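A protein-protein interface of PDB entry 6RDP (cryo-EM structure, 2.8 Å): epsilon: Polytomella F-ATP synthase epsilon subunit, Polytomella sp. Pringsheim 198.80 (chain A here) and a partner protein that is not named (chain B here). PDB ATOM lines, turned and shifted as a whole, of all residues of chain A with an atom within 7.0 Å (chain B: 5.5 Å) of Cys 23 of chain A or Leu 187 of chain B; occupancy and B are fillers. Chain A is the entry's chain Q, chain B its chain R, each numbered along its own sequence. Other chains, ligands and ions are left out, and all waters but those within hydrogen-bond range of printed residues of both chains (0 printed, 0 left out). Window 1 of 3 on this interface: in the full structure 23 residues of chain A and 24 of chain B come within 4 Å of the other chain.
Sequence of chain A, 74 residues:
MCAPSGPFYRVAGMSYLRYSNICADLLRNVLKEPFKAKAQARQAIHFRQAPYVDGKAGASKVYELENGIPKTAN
The side-chain hydroxyl (OG) of Ser 130 of chain B sits close to the backbone carbonyl oxygen (O) of Cys 23 of chain A, at 3.4 Å. The backbone NH (N) of Ala 24 of chain A lies within hydrogen-bond range of the side-chain hydroxyl (OG) of Ser 130 of chain B (3.0 Å). O of Leu 26 of chain A is in hydrogen-bond range of OH of Tyr 188 of chain B.
The side-chain sulfur (SG) of Cys 23 of chain A sits at hydrogen-bond distance from the backbone carbonyl oxygen (O) of Tyr 19 of chain A, at 3.4 Å.
Of the 15 printed residues of chain A, 8 touch a printed residue of chain B. Hydrophobic or aromatic side chains of chain A within 4 Å of the printed part of chain B: Phe 8, Tyr 19, Ala 24, Leu 26, Leu 27 and Val 30. Hydrophobic or aromatic side chains of chain B that line the printed part of chain A: Phe 128, Ala 183, Ala 184, Leu 187, Tyr 188 and Leu 191. Among the printed residues, no Asp or Glu carboxylate lies within 4 Å of a Lys or Arg side-chain nitrogen of the other chain.
Of chain B, only Ser 130 (3.1 Å), Ala 183 (3.9 Å) and Leu 187 (3.3 Å) come within 4 Å of Cys 23 of chain A. Leu 187 of chain B touches just these residues of chain A: Cys 23 (3.3 Å), Leu 26 (3.7 Å) and Leu 27 (3.97 Å). Printed residues of chain A within 4 Å of Leu 191 of chain B: Val 30. Of the printed residues of chain B, Ala 24 of chain A touches Ser 130. Printed residues of chain A within 4 Å of Arg 182 of chain B: Phe 8. Of the printed residues of chain A, Phe 128 of chain B touches Leu 27. Arg 28 of chain A touches none of the printed residues of chain B. Asp 25 of chain A touches none of the printed residues of chain B. The nearest residue of chain A that does not touch Leu 187 of chain B is Ile 22 of chain A (5.1 Å). The nearest printed residue of chain B that does not touch Leu 27 of chain A is Tyr 188 of chain B (5.3 Å).
Among the printed residues, merely in contact across the chains: Cys 23 of chain A with Leu 187 of chain B, Phe 8 of chain A with Arg 182 of chain B, Leu 27 of chain A with Val 129 of chain B, Val 30 of chain A with Tyr 188 of chain B, Leu 27 of chain A with Phe 128 of chain B, Leu 27 of chain A with Ser 130 of chain B, Leu 26 of chain A with Leu 187 of chain B, Tyr 19 of chain A with Ala 183 of chain B, Val 30 of chain A with Leu 191 of chain B, Leu 26 of chain A with Ala 184 of chain B, Ser 20 of chain A with Ser 130 of chain B, Cys 23 of chain A with Ala 183 of chain B and Leu 27 of chain A with Leu 187 of chain B.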
ATOM      1  N   PHE A   8      25.744 -30.886 -12.388  1.00  0.00           N
ATOM      2  CA  PHE A   8      25.199 -31.911 -13.271  1.00  0.00           C
ATOM      3  C   PHE A   8      26.099 -32.189 -14.461  1.00  0.00           C
ATOM      4  O   PHE A   8      26.034 -33.277 -15.039  1.00  0.00           O
ATOM      5  CB  PHE A   8      23.802 -31.517 -13.743  1.00  0.00           C
ATOM      6  CG  PHE A   8      23.772 -30.360 -14.698  1.00  0.00           C
ATOM      7  CD1 PHE A   8      23.600 -30.572 -16.053  1.00  0.00           C
ATOM      8  CD2 PHE A   8      23.863 -29.057 -14.236  1.00  0.00           C
ATOM      9  CE1 PHE A   8      23.555 -29.511 -16.932  1.00  0.00           C
ATOM     10  CE2 PHE A   8      23.820 -27.993 -15.109  1.00  0.00           C
ATOM     11  CZ  PHE A   8      23.663 -28.222 -16.458  1.00  0.00           C
ATOM     12  N   LEU A  17      34.376 -26.418 -18.992  1.00  0.00           N
ATOM     13  CA  LEU A  17      34.585 -25.639 -20.207  1.00  0.00           C
ATOM     14  C   LEU A  17      33.778 -26.192 -21.364  1.00  0.00           C
ATOM     15  O   LEU A  17      33.264 -25.428 -22.189  1.00  0.00           O
ATOM     16  CB  LEU A  17      36.063 -25.616 -20.562  1.00  0.00           C
ATOM     17  CG  LEU A  17      36.818 -24.387 -20.080  1.00  0.00           C
ATOM     18  CD1 LEU A  17      38.197 -24.431 -20.662  1.00  0.00           C
ATOM     19  CD2 LEU A  17      36.103 -23.105 -20.474  1.00  0.00           C
ATOM     20  N   ARG A  18      33.609 -27.512 -21.409  1.00  0.00           N
ATOM     21  CA  ARG A  18      32.783 -28.108 -22.448  1.00  0.00           C
ATOM     22  C   ARG A  18      31.317 -27.759 -22.256  1.00  0.00           C
ATOM     23  O   ARG A  18      30.615 -27.485 -23.229  1.00  0.00           O
ATOM     24  CB  ARG A  18      32.961 -29.617 -22.464  1.00  0.00           C
ATOM     25  CG  ARG A  18      32.528 -30.229 -23.769  1.00  0.00           C
ATOM     26  CD  ARG A  18      32.883 -31.690 -23.817  1.00  0.00           C
ATOM     27  NE  ARG A  18      34.262 -31.930 -24.204  1.00  0.00           N
ATOM     28  CZ  ARG A  18      34.649 -32.118 -25.458  1.00  0.00           C
ATOM     29  NH1 ARG A  18      33.757 -32.085 -26.437  1.00  0.00           N
ATOM     30  NH2 ARG A  18      35.924 -32.339 -25.729  1.00  0.00           N
ATOM     31  N   TYR A  19      30.850 -27.737 -21.007  1.00  0.00           N
ATOM     32  CA  TYR A  19      29.462 -27.389 -20.734  1.00  0.00           C
ATOM     33  C   TYR A  19      29.190 -25.929 -21.061  1.00  0.00           C
ATOM     34  O   TYR A  19      28.167 -25.594 -21.672  1.00  0.00           O
ATOM     35  CB  TYR A  19      29.135 -27.686 -19.272  1.00  0.00           C
ATOM     36  CG  TYR A  19      28.068 -26.803 -18.676  1.00  0.00           C
ATOM     37  CD1 TYR A  19      28.402 -25.770 -17.806  1.00  0.00           C
ATOM     38  CD2 TYR A  19      26.728 -27.011 -18.964  1.00  0.00           C
ATOM     39  CE1 TYR A  19      27.438 -24.964 -17.259  1.00  0.00           C
ATOM     40  CE2 TYR A  19      25.756 -26.208 -18.416  1.00  0.00           C
ATOM     41  CZ  TYR A  19      26.117 -25.184 -17.566  1.00  0.00           C
ATOM     42  OH  TYR A  19      25.154 -24.375 -17.013  1.00  0.00           O
ATOM     43  N   SER A  20      30.107 -25.049 -20.671  1.00  0.00           N
ATOM     44  CA  SER A  20      29.905 -23.632 -20.918  1.00  0.00           C
ATOM     45  C   SER A  20      30.029 -23.314 -22.398  1.00  0.00           C
ATOM     46  O   SER A  20      29.304 -22.455 -22.907  1.00  0.00           O
ATOM     47  CB  SER A  20      30.893 -22.816 -20.095  1.00  0.00           C
ATOM     48  OG  SER A  20      30.594 -21.437 -20.176  1.00  0.00           O
ATOM     49  N   ASN A  21      30.878 -24.042 -23.124  1.00  0.00           N
ATOM     50  CA  ASN A  21      30.952 -23.835 -24.563  1.00  0.00           C
ATOM     51  C   ASN A  21      29.769 -24.457 -25.289  1.00  0.00           C
ATOM     52  O   ASN A  21      29.372 -23.955 -26.339  1.00  0.00           O
ATOM     53  CB  ASN A  21      32.266 -24.385 -25.095  1.00  0.00           C
ATOM     54  CG  ASN A  21      33.364 -23.361 -25.054  1.00  0.00           C
ATOM     55  OD1 ASN A  21      33.340 -22.381 -25.794  1.00  0.00           O
ATOM     56  ND2 ASN A  21      34.316 -23.555 -24.160  1.00  0.00           N
ATOM     57  N   ILE A  22      29.187 -25.529 -24.745  1.00  0.00           N
ATOM     58  CA  ILE A  22      27.958 -26.090 -25.297  1.00  0.00           C
ATOM     59  C   ILE A  22      26.821 -25.091 -25.158  1.00  0.00           C
ATOM     60  O   ILE A  22      26.041 -24.872 -26.097  1.00  0.00           O
ATOM     61  CB  ILE A  22      27.640 -27.435 -24.612  1.00  0.00           C
ATOM     62  CG1 ILE A  22      28.366 -28.578 -25.305  1.00  0.00           C
ATOM     63  CG2 ILE A  22      26.161 -27.747 -24.611  1.00  0.00           C
ATOM     64  CD1 ILE A  22      28.370 -29.850 -24.514  1.00  0.00           C
ATOM     65  N   CYS A  23      26.743 -24.435 -23.998  1.00  0.00           N
ATOM     66  CA  CYS A  23      25.742 -23.391 -23.796  1.00  0.00           C
ATOM     67  C   CYS A  23      25.999 -22.187 -24.696  1.00  0.00           C
ATOM     68  O   CYS A  23      25.055 -21.582 -25.219  1.00  0.00           O
ATOM     69  CB  CYS A  23      25.717 -22.974 -22.329  1.00  0.00           C
ATOM     70  SG  CYS A  23      25.041 -24.213 -21.228  1.00  0.00           S
ATOM     71  N   ALA A  24      27.271 -21.839 -24.906  1.00  0.00           N
ATOM     72  CA  ALA A  24      27.604 -20.748 -25.818  1.00  0.00           C
ATOM     73  C   ALA A  24      27.237 -21.093 -27.256  1.00  0.00           C
ATOM     74  O   ALA A  24      26.747 -20.238 -28.001  1.00  0.00           O
ATOM     75  CB  ALA A  24      29.088 -20.421 -25.707  1.00  0.00           C
ATOM     76  N   ASP A  25      27.418 -22.356 -27.637  1.00  0.00           N
ATOM     77  CA  ASP A  25      27.102 -22.802 -28.989  1.00  0.00           C
ATOM     78  C   ASP A  25      25.599 -22.797 -29.229  1.00  0.00           C
ATOM     79  O   ASP A  25      25.123 -22.382 -30.296  1.00  0.00           O
ATOM     80  CB  ASP A  25      27.676 -24.199 -29.207  1.00  0.00           C
ATOM     81  CG  ASP A  25      29.121 -24.169 -29.647  1.00  0.00           C
ATOM     82  OD1 ASP A  25      29.712 -25.253 -29.826  1.00  0.00           O
ATOM     83  OD2 ASP A  25      29.674 -23.061 -29.802  1.00  0.00           O
ATOM     84  N   LEU A  26      24.835 -23.254 -28.239  1.00  0.00           N
ATOM     85  CA  LEU A  26      23.388 -23.247 -28.369  1.00  0.00           C
ATOM     86  C   LEU A  26      22.800 -21.848 -28.256  1.00  0.00           C
ATOM     87  O   LEU A  26      21.692 -21.624 -28.749  1.00  0.00           O
ATOM     88  CB  LEU A  26      22.777 -24.179 -27.331  1.00  0.00           C
ATOM     89  CG  LEU A  26      23.148 -25.638 -27.594  1.00  0.00           C
ATOM     90  CD1 LEU A  26      22.715 -26.537 -26.454  1.00  0.00           C
ATOM     91  CD2 LEU A  26      22.536 -26.097 -28.904  1.00  0.00           C
ATOM     92  N   LEU A  27      23.505 -20.900 -27.636  1.00  0.00           N
ATOM     93  CA  LEU A  27      23.057 -19.516 -27.738  1.00  0.00           C
ATOM     94  C   LEU A  27      23.406 -18.949 -29.102  1.00  0.00           C
ATOM     95  O   LEU A  27      22.697 -18.081 -29.620  1.00  0.00           O
ATOM     96  CB  LEU A  27      23.686 -18.659 -26.641  1.00  0.00           C
ATOM     97  CG  LEU A  27      23.065 -17.301 -26.260  1.00  0.00           C
ATOM     98  CD1 LEU A  27      23.482 -17.005 -24.852  1.00  0.00           C
ATOM     99  CD2 LEU A  27      23.426 -16.110 -27.132  1.00  0.00           C
ATOM    100  N   ARG A  28      24.509 -19.412 -29.690  1.00  0.00           N
ATOM    101  CA  ARG A  28      24.929 -18.890 -30.985  1.00  0.00           C
ATOM    102  C   ARG A  28      24.017 -19.360 -32.106  1.00  0.00           C
ATOM    103  O   ARG A  28      23.732 -18.591 -33.031  1.00  0.00           O
ATOM    104  CB  ARG A  28      26.374 -19.300 -31.266  1.00  0.00           C
ATOM    105  CG  ARG A  28      27.409 -18.371 -30.659  1.00  0.00           C
ATOM    106  CD  ARG A  28      28.822 -18.824 -30.969  1.00  0.00           C
ATOM    107  NE  ARG A  28      29.794 -18.261 -30.046  1.00  0.00           N
ATOM    108  CZ  ARG A  28      30.588 -18.985 -29.272  1.00  0.00           C
ATOM    109  NH1 ARG A  28      30.540 -20.309 -29.320  1.00  0.00           N
ATOM    110  NH2 ARG A  28      31.439 -18.384 -28.457  1.00  0.00           N
ATOM    111  N   VAL A  30      20.920 -19.680 -32.352  1.00  0.00           N
ATOM    112  CA  VAL A  30      19.579 -19.106 -32.398  1.00  0.00           C
ATOM    113  C   VAL A  30      19.656 -17.592 -32.529  1.00  0.00           C
ATOM    114  O   VAL A  30      18.685 -16.879 -32.247  1.00  0.00           O
ATOM    115  CB  VAL A  30      18.771 -19.518 -31.156  1.00  0.00           C
ATOM    116  CG1 VAL A  30      18.634 -21.025 -31.088  1.00  0.00           C
ATOM    117  CG2 VAL A  30      19.464 -19.029 -29.905  1.00  0.00           C
ATOM    118  N   ILE A  69      31.909 -27.062 -30.581  1.00  0.00           N
ATOM    119  CA  ILE A  69      32.513 -28.088 -29.735  1.00  0.00           C
ATOM    120  C   ILE A  69      31.707 -29.358 -30.006  1.00  0.00           C
ATOM    121  O   ILE A  69      30.548 -29.255 -30.435  1.00  0.00           O
ATOM    122  CB  ILE A  69      32.514 -27.626 -28.261  1.00  0.00           C
ATOM    123  CG1 ILE A  69      33.657 -28.242 -27.448  1.00  0.00           C
ATOM    124  CG2 ILE A  69      31.187 -27.894 -27.579  1.00  0.00           C
ATOM    125  CD1 ILE A  69      34.086 -27.413 -26.264  1.00  0.00           C
ATOM    126  N   PRO B 113      22.273 -19.250 -17.477  1.00  0.00           N
ATOM    127  CA  PRO B 113      21.911 -18.434 -18.643  1.00  0.00           C
ATOM    128  C   PRO B 113      20.744 -17.495 -18.403  1.00  0.00           C
ATOM    129  O   PRO B 113      19.605 -17.934 -18.250  1.00  0.00           O
ATOM    130  CB  PRO B 113      21.557 -19.486 -19.693  1.00  0.00           C
ATOM    131  CG  PRO B 113      22.410 -20.621 -19.352  1.00  0.00           C
ATOM    132  CD  PRO B 113      22.486 -20.657 -17.863  1.00  0.00           C
ATOM    133  N   PHE B 128      21.699 -10.892 -22.889  1.00  0.00           N
ATOM    134  CA  PHE B 128      21.448 -12.273 -22.515  1.00  0.00           C
ATOM    135  C   PHE B 128      22.733 -13.064 -22.697  1.00  0.00           C
ATOM    136  O   PHE B 128      23.253 -13.160 -23.812  1.00  0.00           O
ATOM    137  CB  PHE B 128      20.330 -12.892 -23.342  1.00  0.00           C
ATOM    138  CG  PHE B 128      20.039 -14.316 -22.980  1.00  0.00           C
ATOM    139  CD1 PHE B 128      19.365 -14.619 -21.811  1.00  0.00           C
ATOM    140  CD2 PHE B 128      20.431 -15.349 -23.805  1.00  0.00           C
ATOM    141  CE1 PHE B 128      19.095 -15.928 -21.471  1.00  0.00           C
ATOM    142  CE2 PHE B 128      20.164 -16.659 -23.468  1.00  0.00           C
ATOM    143  CZ  PHE B 128      19.493 -16.946 -22.299  1.00  0.00           C
ATOM    144  N   VAL B 129      23.233 -13.641 -21.611  1.00  0.00           N
ATOM    145  CA  VAL B 129      24.515 -14.319 -21.622  1.00  0.00           C
ATOM    146  C   VAL B 129      24.291 -15.822 -21.586  1.00  0.00           C
ATOM    147  O   VAL B 129      23.172 -16.310 -21.449  1.00  0.00           O
ATOM    148  CB  VAL B 129      25.417 -13.862 -20.466  1.00  0.00           C
ATOM    149  CG1 VAL B 129      25.551 -12.365 -20.496  1.00  0.00           C
ATOM    150  CG2 VAL B 129      24.866 -14.323 -19.152  1.00  0.00           C
ATOM    151  N   SER B 130      25.382 -16.556 -21.741  1.00  0.00           N
ATOM    152  CA  SER B 130      25.377 -18.007 -21.804  1.00  0.00           C
ATOM    153  C   SER B 130      25.685 -18.653 -20.468  1.00  0.00           C
ATOM    154  O   SER B 130      25.692 -19.883 -20.369  1.00  0.00           O
ATOM    155  CB  SER B 130      26.387 -18.473 -22.843  1.00  0.00           C
ATOM    156  OG  SER B 130      26.571 -19.866 -22.762  1.00  0.00           O
ATOM    157  N   ARG B 182      19.927 -31.405 -20.820  1.00  0.00           N
ATOM    158  CA  ARG B 182      19.469 -30.624 -19.676  1.00  0.00           C
ATOM    159  C   ARG B 182      19.909 -29.174 -19.792  1.00  0.00           C
ATOM    160  O   ARG B 182      19.100 -28.256 -19.592  1.00  0.00           O
ATOM    161  CB  ARG B 182      19.999 -31.244 -18.380  1.00  0.00           C
ATOM    162  CG  ARG B 182      19.737 -30.422 -17.129  1.00  0.00           C
ATOM    163  CD  ARG B 182      20.009 -31.240 -15.883  1.00  0.00           C
ATOM    164  NE  ARG B 182      20.099 -30.412 -14.685  1.00  0.00           N
ATOM    165  CZ  ARG B 182      20.318 -30.888 -13.463  1.00  0.00           C
ATOM    166  NH1 ARG B 182      20.473 -32.191 -13.273  1.00  0.00           N
ATOM    167  NH2 ARG B 182      20.386 -30.060 -12.430  1.00  0.00           N
ATOM    168  N   ALA B 183      21.181 -28.959 -20.146  1.00  0.00           N
ATOM    169  CA  ALA B 183      21.679 -27.608 -20.388  1.00  0.00           C
ATOM    170  C   ALA B 183      20.961 -26.956 -21.563  1.00  0.00           C
ATOM    171  O   ALA B 183      20.663 -25.756 -21.527  1.00  0.00           O
ATOM    172  CB  ALA B 183      23.184 -27.647 -20.633  1.00  0.00           C
ATOM    173  N   ALA B 184      20.627 -27.752 -22.584  1.00  0.00           N
ATOM    174  CA  ALA B 184      19.921 -27.248 -23.754  1.00  0.00           C
ATOM    175  C   ALA B 184      18.518 -26.777 -23.409  1.00  0.00           C
ATOM    176  O   ALA B 184      18.135 -25.656 -23.764  1.00  0.00           O
ATOM    177  CB  ALA B 184      19.860 -28.335 -24.825  1.00  0.00           C
ATOM    178  N   ILE B 185      17.747 -27.608 -22.701  1.00  0.00           N
ATOM    179  CA  ILE B 185      16.372 -27.245 -22.379  1.00  0.00           C
ATOM    180  C   ILE B 185      16.342 -26.122 -21.355  1.00  0.00           C
ATOM    181  O   ILE B 185      15.450 -25.270 -21.392  1.00  0.00           O
ATOM    182  CB  ILE B 185      15.555 -28.471 -21.915  1.00  0.00           C
ATOM    183  CG1 ILE B 185      16.103 -29.082 -20.625  1.00  0.00           C
ATOM    184  CG2 ILE B 185      15.497 -29.525 -23.009  1.00  0.00           C
ATOM    185  CD1 ILE B 185      15.201 -30.138 -20.018  1.00  0.00           C
ATOM    186  N   GLU B 186      17.359 -26.035 -20.491  1.00  0.00           N
ATOM    187  CA  GLU B 186      17.355 -24.987 -19.481  1.00  0.00           C
ATOM    188  C   GLU B 186      17.751 -23.639 -20.065  1.00  0.00           C
ATOM    189  O   GLU B 186      17.101 -22.629 -19.767  1.00  0.00           O
ATOM    190  CB  GLU B 186      18.280 -25.394 -18.339  1.00  0.00           C
ATOM    191  CG  GLU B 186      18.170 -24.536 -17.109  1.00  0.00           C
ATOM    192  CD  GLU B 186      18.954 -25.111 -15.951  1.00  0.00           C
ATOM    193  OE1 GLU B 186      19.655 -26.125 -16.151  1.00  0.00           O
ATOM    194  OE2 GLU B 186      18.845 -24.568 -14.835  1.00  0.00           O
ATOM    195  N   LEU B 187      18.769 -23.614 -20.932  1.00  0.00           N
ATOM    196  CA  LEU B 187      19.142 -22.390 -21.634  1.00  0.00           C
ATOM    197  C   LEU B 187      18.038 -21.933 -22.574  1.00  0.00           C
ATOM    198  O   LEU B 187      17.724 -20.739 -22.641  1.00  0.00           O
ATOM    199  CB  LEU B 187      20.437 -22.623 -22.406  1.00  0.00           C
ATOM    200  CG  LEU B 187      20.794 -21.738 -23.601  1.00  0.00           C
ATOM    201  CD1 LEU B 187      21.028 -20.271 -23.263  1.00  0.00           C
ATOM    202  CD2 LEU B 187      22.011 -22.325 -24.249  1.00  0.00           C
ATOM    203  N   TYR B 188      17.434 -22.871 -23.311  1.00  0.00           N
ATOM    204  CA  TYR B 188      16.372 -22.511 -24.238  1.00  0.00           C
ATOM    205  C   TYR B 188      15.121 -22.049 -23.507  1.00  0.00           C
ATOM    206  O   TYR B 188      14.452 -21.113 -23.962  1.00  0.00           O
ATOM    207  CB  TYR B 188      16.072 -23.700 -25.143  1.00  0.00           C
ATOM    208  CG  TYR B 188      17.010 -23.804 -26.311  1.00  0.00           C
ATOM    209  CD1 TYR B 188      17.574 -22.666 -26.865  1.00  0.00           C
ATOM    210  CD2 TYR B 188      17.354 -25.037 -26.845  1.00  0.00           C
ATOM    211  CE1 TYR B 188      18.434 -22.746 -27.932  1.00  0.00           C
ATOM    212  CE2 TYR B 188      18.220 -25.130 -27.916  1.00  0.00           C
ATOM    213  CZ  TYR B 188      18.755 -23.978 -28.456  1.00  0.00           C
ATOM    214  OH  TYR B 188      19.620 -24.043 -29.522  1.00  0.00           O
ATOM    215  N   SER B 189      14.820 -22.652 -22.357  1.00  0.00           N
ATOM    216  CA  SER B 189      13.682 -22.224 -21.564  1.00  0.00           C
ATOM    217  C   SER B 189      13.912 -20.843 -20.969  1.00  0.00           C
ATOM    218  O   SER B 189      12.993 -20.017 -20.936  1.00  0.00           O
ATOM    219  CB  SER B 189      13.427 -23.252 -20.470  1.00  0.00           C
ATOM    220  OG  SER B 189      13.230 -24.534 -21.037  1.00  0.00           O
ATOM    221  N   ALA B 190      15.136 -20.568 -20.509  1.00  0.00           N
ATOM    222  CA  ALA B 190      15.441 -19.241 -19.993  1.00  0.00           C
ATOM    223  C   ALA B 190      15.428 -18.190 -21.095  1.00  0.00           C
ATOM    224  O   ALA B 190      14.996 -17.056 -20.861  1.00  0.00           O
ATOM    225  CB  ALA B 190      16.793 -19.258 -19.290  1.00  0.00           C
ATOM    226  N   LEU B 191      15.856 -18.565 -22.302  1.00  0.00           N
ATOM    227  CA  LEU B 191      15.795 -17.653 -23.441  1.00  0.00           C
ATOM    228  C   LEU B 191      14.355 -17.346 -23.829  1.00  0.00           C
ATOM    229  O   LEU B 191      14.018 -16.192 -24.128  1.00  0.00           O
ATOM    230  CB  LEU B 191      16.554 -18.258 -24.620  1.00  0.00           C
ATOM    231  CG  LEU B 191      16.757 -17.387 -25.856  1.00  0.00           C
ATOM    232  CD1 LEU B 191      17.203 -15.982 -25.487  1.00  0.00           C
ATOM    233  CD2 LEU B 191      17.770 -18.051 -26.751  1.00  0.00           C
ATOM    234  N   GLU B 192      13.492 -18.365 -23.809  1.00  0.00           N
ATOM    235  CA  GLU B 192      12.072 -18.168 -24.087  1.00  0.00           C
ATOM    236  C   GLU B 192      11.424 -17.274 -23.039  1.00  0.00           C
ATOM    237  O   GLU B 192      10.737 -16.300 -23.374  1.00  0.00           O
ATOM    238  CB  GLU B 192      11.366 -19.520 -24.146  1.00  0.00           C
ATOM    239  CG  GLU B 192      11.523 -20.233 -25.467  1.00  0.00           C
ATOM    240  CD  GLU B 192      11.577 -21.731 -25.306  1.00  0.00           C
ATOM    241  OE1 GLU B 192      11.173 -22.222 -24.237  1.00  0.00           O
ATOM    242  OE2 GLU B 192      12.027 -22.420 -26.241  1.00  0.00           O
